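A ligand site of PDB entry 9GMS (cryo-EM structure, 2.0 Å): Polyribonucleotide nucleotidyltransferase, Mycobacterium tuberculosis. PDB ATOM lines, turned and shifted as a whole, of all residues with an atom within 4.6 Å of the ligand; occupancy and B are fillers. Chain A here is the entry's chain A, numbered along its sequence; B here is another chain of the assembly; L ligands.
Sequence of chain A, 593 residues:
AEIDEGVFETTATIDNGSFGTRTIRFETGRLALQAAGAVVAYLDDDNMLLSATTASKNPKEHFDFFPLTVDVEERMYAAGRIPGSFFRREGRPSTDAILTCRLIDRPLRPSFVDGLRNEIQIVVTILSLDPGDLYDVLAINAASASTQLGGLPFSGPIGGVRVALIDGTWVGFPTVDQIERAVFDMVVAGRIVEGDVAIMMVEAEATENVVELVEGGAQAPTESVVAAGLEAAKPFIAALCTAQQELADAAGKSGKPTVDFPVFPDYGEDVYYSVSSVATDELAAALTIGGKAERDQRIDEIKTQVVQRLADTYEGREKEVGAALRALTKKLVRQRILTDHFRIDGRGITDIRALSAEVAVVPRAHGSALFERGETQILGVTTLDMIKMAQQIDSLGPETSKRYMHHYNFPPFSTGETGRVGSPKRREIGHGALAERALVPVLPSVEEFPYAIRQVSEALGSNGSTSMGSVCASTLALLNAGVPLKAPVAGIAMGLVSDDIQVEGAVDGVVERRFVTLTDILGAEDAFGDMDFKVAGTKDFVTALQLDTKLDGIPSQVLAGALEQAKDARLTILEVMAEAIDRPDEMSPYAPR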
ATOM      1  N   LEU A 287     -16.421   0.703  -0.660  1.00  0.00           N
ATOM      2  CA  LEU A 287     -17.745   0.159  -0.390  1.00  0.00           C
ATOM      3  C   LEU A 287     -18.785   1.234  -0.126  1.00  0.00           C
ATOM      4  O   LEU A 287     -19.980   0.935  -0.123  1.00  0.00           O
ATOM      5  CB  LEU A 287     -17.694  -0.790   0.798  1.00  0.00           C
ATOM      6  CG  LEU A 287     -16.981  -2.131   0.563  1.00  0.00           C
ATOM      7  CD1 LEU A 287     -16.773  -2.848   1.880  1.00  0.00           C
ATOM      8  CD2 LEU A 287     -17.782  -2.990  -0.391  1.00  0.00           C
ATOM      9  N   ARG A 295     -18.285   1.579  -8.223  1.00  0.00           N
ATOM     10  CA  ARG A 295     -17.769   0.737  -7.150  1.00  0.00           C
ATOM     11  C   ARG A 295     -16.985  -0.447  -7.710  1.00  0.00           C
ATOM     12  O   ARG A 295     -15.904  -0.779  -7.207  1.00  0.00           O
ATOM     13  CB  ARG A 295     -18.923   0.265  -6.259  1.00  0.00           C
ATOM     14  CG  ARG A 295     -18.545  -0.856  -5.316  1.00  0.00           C
ATOM     15  CD  ARG A 295     -19.485  -0.946  -4.133  1.00  0.00           C
ATOM     16  NE  ARG A 295     -20.887  -0.874  -4.531  1.00  0.00           N
ATOM     17  CZ  ARG A 295     -21.570  -1.893  -5.040  1.00  0.00           C
ATOM     18  NH1 ARG A 295     -21.014  -3.067  -5.243  1.00  0.00           N
ATOM     19  NH2 ARG A 295     -22.851  -1.706  -5.362  1.00  0.00           N
ATOM     20  N   ILE A 299     -12.981  -1.146  -7.077  1.00  0.00           N
ATOM     21  CA  ILE A 299     -12.497  -2.375  -6.475  1.00  0.00           C
ATOM     22  C   ILE A 299     -11.506  -3.065  -7.409  1.00  0.00           C
ATOM     23  O   ILE A 299     -10.484  -3.595  -6.962  1.00  0.00           O
ATOM     24  CB  ILE A 299     -13.681  -3.301  -6.117  1.00  0.00           C
ATOM     25  CG1 ILE A 299     -14.478  -2.665  -4.978  1.00  0.00           C
ATOM     26  CG2 ILE A 299     -13.176  -4.677  -5.713  1.00  0.00           C
ATOM     27  CD1 ILE A 299     -15.678  -3.469  -4.548  1.00  0.00           C
ATOM     28  N   LYS A 303      -7.625  -3.886  -6.512  1.00  0.00           N
ATOM     29  CA  LYS A 303      -7.127  -5.246  -6.611  1.00  0.00           C
ATOM     30  C   LYS A 303      -5.915  -5.323  -7.542  1.00  0.00           C
ATOM     31  O   LYS A 303      -4.926  -5.983  -7.217  1.00  0.00           O
ATOM     32  CB  LYS A 303      -8.270  -6.170  -7.071  1.00  0.00           C
ATOM     33  CG  LYS A 303      -7.864  -7.539  -7.617  1.00  0.00           C
ATOM     34  CD  LYS A 303      -9.068  -8.399  -8.110  1.00  0.00           C
ATOM     35  CE  LYS A 303     -10.468  -7.827  -7.798  1.00  0.00           C
ATOM     36  NZ  LYS A 303     -11.545  -8.736  -8.308  1.00  0.00           N
ATOM     37  N   GLY A 322      -5.104 -12.588  -4.036  1.00  0.00           N
ATOM     38  CA  GLY A 322      -6.509 -12.472  -4.372  1.00  0.00           C
ATOM     39  C   GLY A 322      -7.408 -13.044  -3.305  1.00  0.00           C
ATOM     40  O   GLY A 322      -8.431 -12.441  -2.944  1.00  0.00           O
ATOM     41  N   LEU A 325      -7.525 -10.685  -0.337  1.00  0.00           N
ATOM     42  CA  LEU A 325      -8.351  -9.515  -0.630  1.00  0.00           C
ATOM     43  C   LEU A 325      -9.831  -9.851  -0.532  1.00  0.00           C
ATOM     44  O   LEU A 325     -10.610  -9.075   0.044  1.00  0.00           O
ATOM     45  CB  LEU A 325      -8.010  -8.981  -2.023  1.00  0.00           C
ATOM     46  CG  LEU A 325      -6.876  -7.969  -2.086  1.00  0.00           C
ATOM     47  CD1 LEU A 325      -6.360  -7.848  -3.497  1.00  0.00           C
ATOM     48  CD2 LEU A 325      -7.330  -6.626  -1.565  1.00  0.00           C
ATOM     49  N   ARG A 326     -10.236 -10.994  -1.082  1.00  0.00           N
ATOM     50  CA  ARG A 326     -11.646 -11.372  -1.010  1.00  0.00           C
ATOM     51  C   ARG A 326     -12.089 -11.582   0.431  1.00  0.00           C
ATOM     52  O   ARG A 326     -13.180 -11.142   0.825  1.00  0.00           O
ATOM     53  CB  ARG A 326     -11.894 -12.625  -1.846  1.00  0.00           C
ATOM     54  CG  ARG A 326     -13.289 -13.193  -1.678  1.00  0.00           C
ATOM     55  CD  ARG A 326     -13.741 -14.000  -2.882  1.00  0.00           C
ATOM     56  NE  ARG A 326     -12.651 -14.798  -3.450  1.00  0.00           N
ATOM     57  CZ  ARG A 326     -12.055 -14.571  -4.609  1.00  0.00           C
ATOM     58  NH1 ARG A 326     -12.435 -13.585  -5.409  1.00  0.00           N
ATOM     59  NH2 ARG A 326     -11.060 -15.365  -4.988  1.00  0.00           N
ATOM     60  N   THR A 329     -12.538  -8.232   2.119  1.00  0.00           N
ATOM     61  CA  THR A 329     -13.763  -7.579   1.654  1.00  0.00           C
ATOM     62  C   THR A 329     -14.992  -8.168   2.328  1.00  0.00           C
ATOM     63  O   THR A 329     -15.900  -7.440   2.730  1.00  0.00           O
ATOM     64  CB  THR A 329     -13.873  -7.689   0.136  1.00  0.00           C
ATOM     65  OG1 THR A 329     -12.660  -7.244  -0.474  1.00  0.00           O
ATOM     66  CG2 THR A 329     -15.034  -6.850  -0.379  1.00  0.00           C
ATOM     67  N   VAL A 333     -17.728  -6.125   4.658  1.00  0.00           N
ATOM     68  CA  VAL A 333     -19.155  -6.077   4.337  1.00  0.00           C
ATOM     69  C   VAL A 333     -19.988  -6.567   5.521  1.00  0.00           C
ATOM     70  O   VAL A 333     -20.980  -5.932   5.919  1.00  0.00           O
ATOM     71  CB  VAL A 333     -19.442  -6.908   3.073  1.00  0.00           C
ATOM     72  CG1 VAL A 333     -20.937  -7.146   2.911  1.00  0.00           C
ATOM     73  CG2 VAL A 333     -18.893  -6.210   1.840  1.00  0.00           C
ATOM     74  N   ILE A 344     -24.975  -3.365   0.653  1.00  0.00           N
ATOM     75  CA  ILE A 344     -24.077  -2.995  -0.436  1.00  0.00           C
ATOM     76  C   ILE A 344     -24.732  -1.945  -1.336  1.00  0.00           C
ATOM     77  O   ILE A 344     -24.084  -0.968  -1.739  1.00  0.00           O
ATOM     78  CB  ILE A 344     -23.663  -4.238  -1.245  1.00  0.00           C
ATOM     79  CG1 ILE A 344     -22.621  -5.041  -0.470  1.00  0.00           C
ATOM     80  CG2 ILE A 344     -23.148  -3.850  -2.610  1.00  0.00           C
ATOM     81  CD1 ILE A 344     -22.396  -6.429  -1.027  1.00  0.00           C
ATOM     82  N   TYR A 408     -36.518 -25.468 -16.217  1.00  0.00           N
ATOM     83  CA  TYR A 408     -35.800 -24.260 -15.854  1.00  0.00           C
ATOM     84  C   TYR A 408     -34.455 -24.215 -16.577  1.00  0.00           C
ATOM     85  O   TYR A 408     -33.732 -25.214 -16.611  1.00  0.00           O
ATOM     86  CB  TYR A 408     -35.613 -24.211 -14.320  1.00  0.00           C
ATOM     87  CG  TYR A 408     -34.578 -23.239 -13.833  1.00  0.00           C
ATOM     88  CD1 TYR A 408     -34.927 -21.937 -13.487  1.00  0.00           C
ATOM     89  CD2 TYR A 408     -33.255 -23.614 -13.685  1.00  0.00           C
ATOM     90  CE1 TYR A 408     -33.989 -21.050 -13.041  1.00  0.00           C
ATOM     91  CE2 TYR A 408     -32.313 -22.719 -13.230  1.00  0.00           C
ATOM     92  CZ  TYR A 408     -32.678 -21.445 -12.902  1.00  0.00           C
ATOM     93  OH  TYR A 408     -31.741 -20.559 -12.457  1.00  0.00           O
ATOM     94  N   PHE A 410     -30.766 -21.907 -17.370  1.00  0.00           N
ATOM     95  CA  PHE A 410     -29.812 -20.932 -16.839  1.00  0.00           C
ATOM     96  C   PHE A 410     -28.642 -20.771 -17.806  1.00  0.00           C
ATOM     97  O   PHE A 410     -27.615 -21.438 -17.662  1.00  0.00           O
ATOM     98  CB  PHE A 410     -29.323 -21.373 -15.451  1.00  0.00           C
ATOM     99  CG  PHE A 410     -28.235 -20.508 -14.883  1.00  0.00           C
ATOM    100  CD1 PHE A 410     -28.476 -19.178 -14.597  1.00  0.00           C
ATOM    101  CD2 PHE A 410     -26.983 -21.022 -14.615  1.00  0.00           C
ATOM    102  CE1 PHE A 410     -27.483 -18.382 -14.067  1.00  0.00           C
ATOM    103  CE2 PHE A 410     -25.986 -20.230 -14.093  1.00  0.00           C
ATOM    104  CZ  PHE A 410     -26.235 -18.904 -13.810  1.00  0.00           C
ATOM    105  N   HIS A 431     -33.468 -26.488  -9.057  1.00  0.00           N
ATOM    106  CA  HIS A 431     -34.253 -25.250  -9.071  1.00  0.00           C
ATOM    107  C   HIS A 431     -35.595 -25.457  -9.760  1.00  0.00           C
ATOM    108  O   HIS A 431     -36.638 -24.976  -9.285  1.00  0.00           O
ATOM    109  CB  HIS A 431     -33.467 -24.134  -9.737  1.00  0.00           C
ATOM    110  CG  HIS A 431     -32.247 -23.712  -8.974  1.00  0.00           C
ATOM    111  ND1 HIS A 431     -32.282 -23.378  -7.643  1.00  0.00           N
ATOM    112  CD2 HIS A 431     -30.951 -23.588  -9.359  1.00  0.00           C
ATOM    113  CE1 HIS A 431     -31.067 -23.058  -7.235  1.00  0.00           C
ATOM    114  NE2 HIS A 431     -30.234 -23.185  -8.257  1.00  0.00           N
ATOM    115  N   SER A 462     -29.522 -12.888 -13.845  1.00  0.00           N
ATOM    116  CA  SER A 462     -29.414 -13.538 -12.546  1.00  0.00           C
ATOM    117  C   SER A 462     -28.569 -12.707 -11.590  1.00  0.00           C
ATOM    118  O   SER A 462     -27.394 -12.460 -11.857  1.00  0.00           O
ATOM    119  CB  SER A 462     -28.819 -14.942 -12.681  1.00  0.00           C
ATOM    120  OG  SER A 462     -29.579 -15.740 -13.558  1.00  0.00           O
ATOM    121  N   ASN A 463     -29.185 -12.255 -10.499  1.00  0.00           N
ATOM    122  CA  ASN A 463     -28.469 -11.643  -9.381  1.00  0.00           C
ATOM    123  C   ASN A 463     -29.098 -12.055  -8.053  1.00  0.00           C
ATOM    124  O   ASN A 463     -29.361 -11.224  -7.185  1.00  0.00           O
ATOM    125  CB  ASN A 463     -28.445 -10.115  -9.517  1.00  0.00           C
ATOM    126  CG  ASN A 463     -27.389  -9.474  -8.627  1.00  0.00           C
ATOM    127  OD1 ASN A 463     -26.452 -10.122  -8.183  1.00  0.00           O
ATOM    128  ND2 ASN A 463     -27.534  -8.180  -8.382  1.00  0.00           N
ATOM    129  N   GLY A 464     -29.375 -13.342  -7.891  1.00  0.00           N
ATOM    130  CA  GLY A 464     -29.890 -13.862  -6.643  1.00  0.00           C
ATOM    131  C   GLY A 464     -31.348 -14.260  -6.675  1.00  0.00           C
ATOM    132  O   GLY A 464     -32.215 -13.471  -7.060  1.00  0.00           O
ATOM    133  N   SER A 465     -31.628 -15.497  -6.248  1.00  0.00           N
ATOM    134  CA  SER A 465     -32.988 -15.984  -6.044  1.00  0.00           C
ATOM    135  C   SER A 465     -33.779 -16.017  -7.356  1.00  0.00           C
ATOM    136  O   SER A 465     -34.807 -15.362  -7.519  1.00  0.00           O
ATOM    137  CB  SER A 465     -33.705 -15.147  -4.993  1.00  0.00           C
ATOM    138  OG  SER A 465     -35.009 -15.628  -4.762  1.00  0.00           O
ATOM    139  N   THR A 466     -33.281 -16.824  -8.288  1.00  0.00           N
ATOM    140  CA  THR A 466     -33.951 -17.010  -9.570  1.00  0.00           C
ATOM    141  C   THR A 466     -35.140 -17.966  -9.481  1.00  0.00           C
ATOM    142  O   THR A 466     -36.066 -17.859 -10.294  1.00  0.00           O
ATOM    143  CB  THR A 466     -32.921 -17.501 -10.601  1.00  0.00           C
ATOM    144  OG1 THR A 466     -31.968 -16.468 -10.866  1.00  0.00           O
ATOM    145  CG2 THR A 466     -33.581 -17.868 -11.860  1.00  0.00           C
ATOM    146  N   SER A 467     -35.151 -18.877  -8.505  1.00  0.00           N
ATOM    147  CA  SER A 467     -36.246 -19.833  -8.390  1.00  0.00           C
ATOM    148  C   SER A 467     -37.542 -19.169  -7.921  1.00  0.00           C
ATOM    149  O   SER A 467     -38.631 -19.499  -8.395  1.00  0.00           O
ATOM    150  CB  SER A 467     -35.843 -20.981  -7.456  1.00  0.00           C
ATOM    151  OG  SER A 467     -35.322 -20.500  -6.226  1.00  0.00           O
ATOM    152  N   GLY A 523     -26.848 -11.726  -4.672  1.00  0.00           N
ATOM    153  CA  GLY A 523     -25.932 -12.851  -4.795  1.00  0.00           C
ATOM    154  C   GLY A 523     -24.739 -12.745  -3.858  1.00  0.00           C
ATOM    155  O   GLY A 523     -24.328 -13.727  -3.237  1.00  0.00           O
ATOM    156  N   ALA A 524     -24.184 -11.534  -3.729  1.00  0.00           N
ATOM    157  CA  ALA A 524     -23.038 -11.346  -2.854  1.00  0.00           C
ATOM    158  C   ALA A 524     -23.409 -11.535  -1.386  1.00  0.00           C
ATOM    159  O   ALA A 524     -22.606 -12.033  -0.603  1.00  0.00           O
ATOM    160  CB  ALA A 524     -22.445  -9.957  -3.081  1.00  0.00           C
ATOM    161  N   ALA A 527     -23.356 -15.100  -0.806  1.00  0.00           N
ATOM    162  CA  ALA A 527     -21.987 -15.615  -0.730  1.00  0.00           C
ATOM    163  C   ALA A 527     -21.337 -15.290   0.613  1.00  0.00           C
ATOM    164  O   ALA A 527     -20.632 -16.128   1.183  1.00  0.00           O
ATOM    165  CB  ALA A 527     -21.164 -15.049  -1.873  1.00  0.00           C
ATOM    166  N   PHE A 528     -21.553 -14.089   1.132  1.00  0.00           N
ATOM    167  CA  PHE A 528     -20.930 -13.651   2.379  1.00  0.00           C
ATOM    168  C   PHE A 528     -21.788 -13.892   3.607  1.00  0.00           C
ATOM    169  O   PHE A 528     -21.335 -13.620   4.717  1.00  0.00           O
ATOM    170  CB  PHE A 528     -20.583 -12.156   2.301  1.00  0.00           C
ATOM    171  CG  PHE A 528     -19.623 -11.794   1.200  1.00  0.00           C
ATOM    172  CD1 PHE A 528     -18.728 -12.717   0.700  1.00  0.00           C
ATOM    173  CD2 PHE A 528     -19.620 -10.519   0.673  1.00  0.00           C
ATOM    174  CE1 PHE A 528     -17.856 -12.371  -0.311  1.00  0.00           C
ATOM    175  CE2 PHE A 528     -18.753 -10.168  -0.330  1.00  0.00           C
ATOM    176  CZ  PHE A 528     -17.870 -11.098  -0.819  1.00  0.00           C
ATOM    177  P     A B   9     -24.017 -20.389  -7.842  1.00  0.00           P
ATOM    178  OP1   A B   9     -24.838 -19.476  -7.024  1.00  0.00           O
ATOM    179  OP2   A B   9     -24.665 -21.538  -8.511  1.00  0.00           O
ATOM    180  O5'   A B   9     -23.252 -19.527  -8.936  1.00  0.00           O
ATOM    181  C5'   A B   9     -23.898 -19.082 -10.117  1.00  0.00           C
ATOM    182  C4'   A B   9     -23.096 -18.009 -10.813  1.00  0.00           C
ATOM    183  O4'   A B   9     -22.985 -16.856  -9.942  1.00  0.00           O
ATOM    184  C3'   A B   9     -21.661 -18.362 -11.159  1.00  0.00           C
ATOM    185  O3'   A B   9     -21.552 -19.073 -12.377  1.00  0.00           O
ATOM    186  C2'   A B   9     -20.962 -17.006 -11.178  1.00  0.00           C
ATOM    187  O2'   A B   9     -21.178 -16.339 -12.406  1.00  0.00           O
ATOM    188  C1'   A B   9     -21.711 -16.272 -10.071  1.00  0.00           C
ATOM    189  N9    A B   9     -21.024 -16.356  -8.774  1.00  0.00           N
ATOM    190  C8    A B   9     -21.383 -17.107  -7.686  1.00  0.00           C
ATOM    191  N7    A B   9     -20.573 -16.979  -6.666  1.00  0.00           N
ATOM    192  C5    A B   9     -19.626 -16.070  -7.107  1.00  0.00           C
ATOM    193  C6    A B   9     -18.497 -15.509  -6.490  1.00  0.00           C
ATOM    194  N6    A B   9     -18.118 -15.788  -5.247  1.00  0.00           N
ATOM    195  N1    A B   9     -17.759 -14.641  -7.216  1.00  0.00           N
ATOM    196  C2    A B   9     -18.147 -14.365  -8.461  1.00  0.00           C
ATOM    197  N3    A B   9     -19.182 -14.824  -9.151  1.00  0.00           N
ATOM    198  C4    A B   9     -19.888 -15.680  -8.401  1.00  0.00           C
HETATM  199  C1  LIG L   1     -19.935 -11.872  -6.117  1.00  0.00           C
HETATM  200  C2  LIG L   1     -22.251 -13.211  -6.957  1.00  0.00           C
HETATM  201  C3  LIG L   1     -24.278 -13.554  -8.552  1.00  0.00           C
HETATM  202  C4  LIG L   1     -25.863 -15.358  -8.244  1.00  0.00           C
HETATM  203  C5  LIG L   1     -28.323 -18.441  -8.640  1.00  0.00           C
HETATM  204  C6  LIG L   1     -29.606 -17.900  -7.909  1.00  0.00           C
HETATM  205  C7  LIG L   1     -28.535 -18.412 -10.338  1.00  0.00           C
HETATM  206  C8  LIG L   1     -28.362 -20.652  -9.577  1.00  0.00           C
HETATM  207  C9  LIG L   1     -18.357  -6.905  -3.785  1.00  0.00           C
HETATM  208  C10 LIG L   1     -17.243  -7.889  -4.256  1.00  0.00           C
HETATM  209  C11 LIG L   1     -17.420  -9.082  -4.972  1.00  0.00           C
HETATM  210  C12 LIG L   1     -18.711  -9.731  -5.460  1.00  0.00           C
HETATM  211  C13 LIG L   1     -20.568 -12.803  -5.282  1.00  0.00           C
HETATM  212  C14 LIG L   1     -21.716 -13.467  -5.706  1.00  0.00           C
HETATM  213  C15 LIG L   1     -23.572 -13.985  -7.437  1.00  0.00           C
HETATM  214  C16 LIG L   1     -25.418 -14.226  -8.954  1.00  0.00           C
HETATM  215  C17 LIG L   1     -27.071 -16.127  -8.625  1.00  0.00           C
HETATM  216  C18 LIG L   1     -28.334 -19.656 -10.826  1.00  0.00           C
HETATM  217  C19 LIG L   1     -28.133 -19.713  -8.266  1.00  0.00           C
HETATM  218  C20 LIG L   1     -25.168 -15.784  -7.137  1.00  0.00           C
HETATM  219  C21 LIG L   1     -24.019 -15.109  -6.733  1.00  0.00           C
HETATM  220  C22 LIG L   1     -21.613 -12.284  -7.799  1.00  0.00           C
HETATM  221  C23 LIG L   1     -20.466 -11.620  -7.375  1.00  0.00           C
HETATM  222  C24 LIG L   1     -15.313  -8.735  -4.573  1.00  0.00           C
HETATM  223  C25 LIG L   1     -13.757  -8.915  -4.529  1.00  0.00           C
HETATM  224  C26 LIG L   1     -13.146 -10.001  -5.167  1.00  0.00           C
HETATM  225  C27 LIG L   1     -11.768 -10.161  -5.117  1.00  0.00           C
HETATM  226  C28 LIG L   1     -10.994  -9.256  -4.425  1.00  0.00           C
HETATM  227  C29 LIG L   1     -11.608  -8.174  -3.773  1.00  0.00           C
HETATM  228  C30 LIG L   1     -12.983  -8.010  -3.837  1.00  0.00           C
HETATM  229  F1  LIG L   1     -19.556  -7.185  -4.441  1.00  0.00           F
HETATM  230  F2  LIG L   1     -18.531  -7.029  -2.453  1.00  0.00           F
HETATM  231  F3  LIG L   1     -17.987  -5.652  -4.055  1.00  0.00           F
HETATM  232  N1  LIG L   1     -18.753 -11.204  -5.662  1.00  0.00           N
HETATM  233  N2  LIG L   1     -27.124 -17.578  -8.281  1.00  0.00           N
HETATM  234  N3  LIG L   1     -16.154  -9.574  -5.136  1.00  0.00           N
HETATM  235  O1  LIG L   1     -15.965  -7.736  -4.048  1.00  0.00           O
HETATM  236  O2  LIG L   1     -30.715 -17.949  -8.472  1.00  0.00           O
HETATM  237  O3  LIG L   1     -29.498 -17.399  -6.715  1.00  0.00           O
HETATM  238  O4  LIG L   1     -27.932 -15.618  -9.164  1.00  0.00           O
HETATM  239  O5  LIG L   1     -19.652  -9.083  -5.673  1.00  0.00           O
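O2 of the ligand is in hydrogen-bond range of N of Thr 466 (2.8 Å). The side-chain hydroxyl of Thr 466 is in hydrogen-bond range of an oxygen (O2) of the ligand (3.1 Å). The backbone NH of Ser 465 is in hydrogen-bond range of an oxygen (O3) of the ligand (2.9 Å). N of Gly 464 sits at hydrogen-bond distance from O4 of the ligand, 3.0 Å away. OP1 of A 9 of chain B is in hydrogen-bond range of N2 of the ligand (3.2 Å).
The side-chain hydroxyl (OG1) of Thr 329 lies within hydrogen-bond range of the backbone carbonyl oxygen (O) of Leu 325 (2.8 Å).
Ile 299 touches the ligand (CD1 to F3, 3.2 Å). Lys 303 touches the ligand. Leu 325 touches the ligand (CB to C28, 3.8 Å). Arg 326 touches the ligand. Thr 329 touches the ligand (OG1 to C30, 3.5 Å). OH of Tyr 408 touches C18 of the ligand, 3.9 Å away. Phe 410 touches the ligand (CE1 to C18, 3.6 Å). NE2 of His 431 touches C8 of the ligand, at 3.4 Å. Ser 462 touches the ligand. N of Asn 463 touches O4 of the ligand, 3.8 Å away. Gly 523 touches the ligand. N of Ala 524 touches C14 of the ligand (3.7 Å). Phe 528 touches the ligand. Hydrophobic or aromatic side chains within 4 Å of the ligand: Ile 299, Leu 325, Phe 410, His 431, Ala 524 and Phe 528. 17 residues have an atom within 4 Å of the ligand: Ile 299, Lys 303, Leu 325, Arg 326, Thr 329, Tyr 408, Phe 410, His 431, Ser 462, Asn 463, Gly 464, Ser 465, Thr 466, Gly 523, Ala 524, Phe 528 and A 9 of chain B. The nearest printed residue that does not touch the ligand is Ala 527 (4.1 Å).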
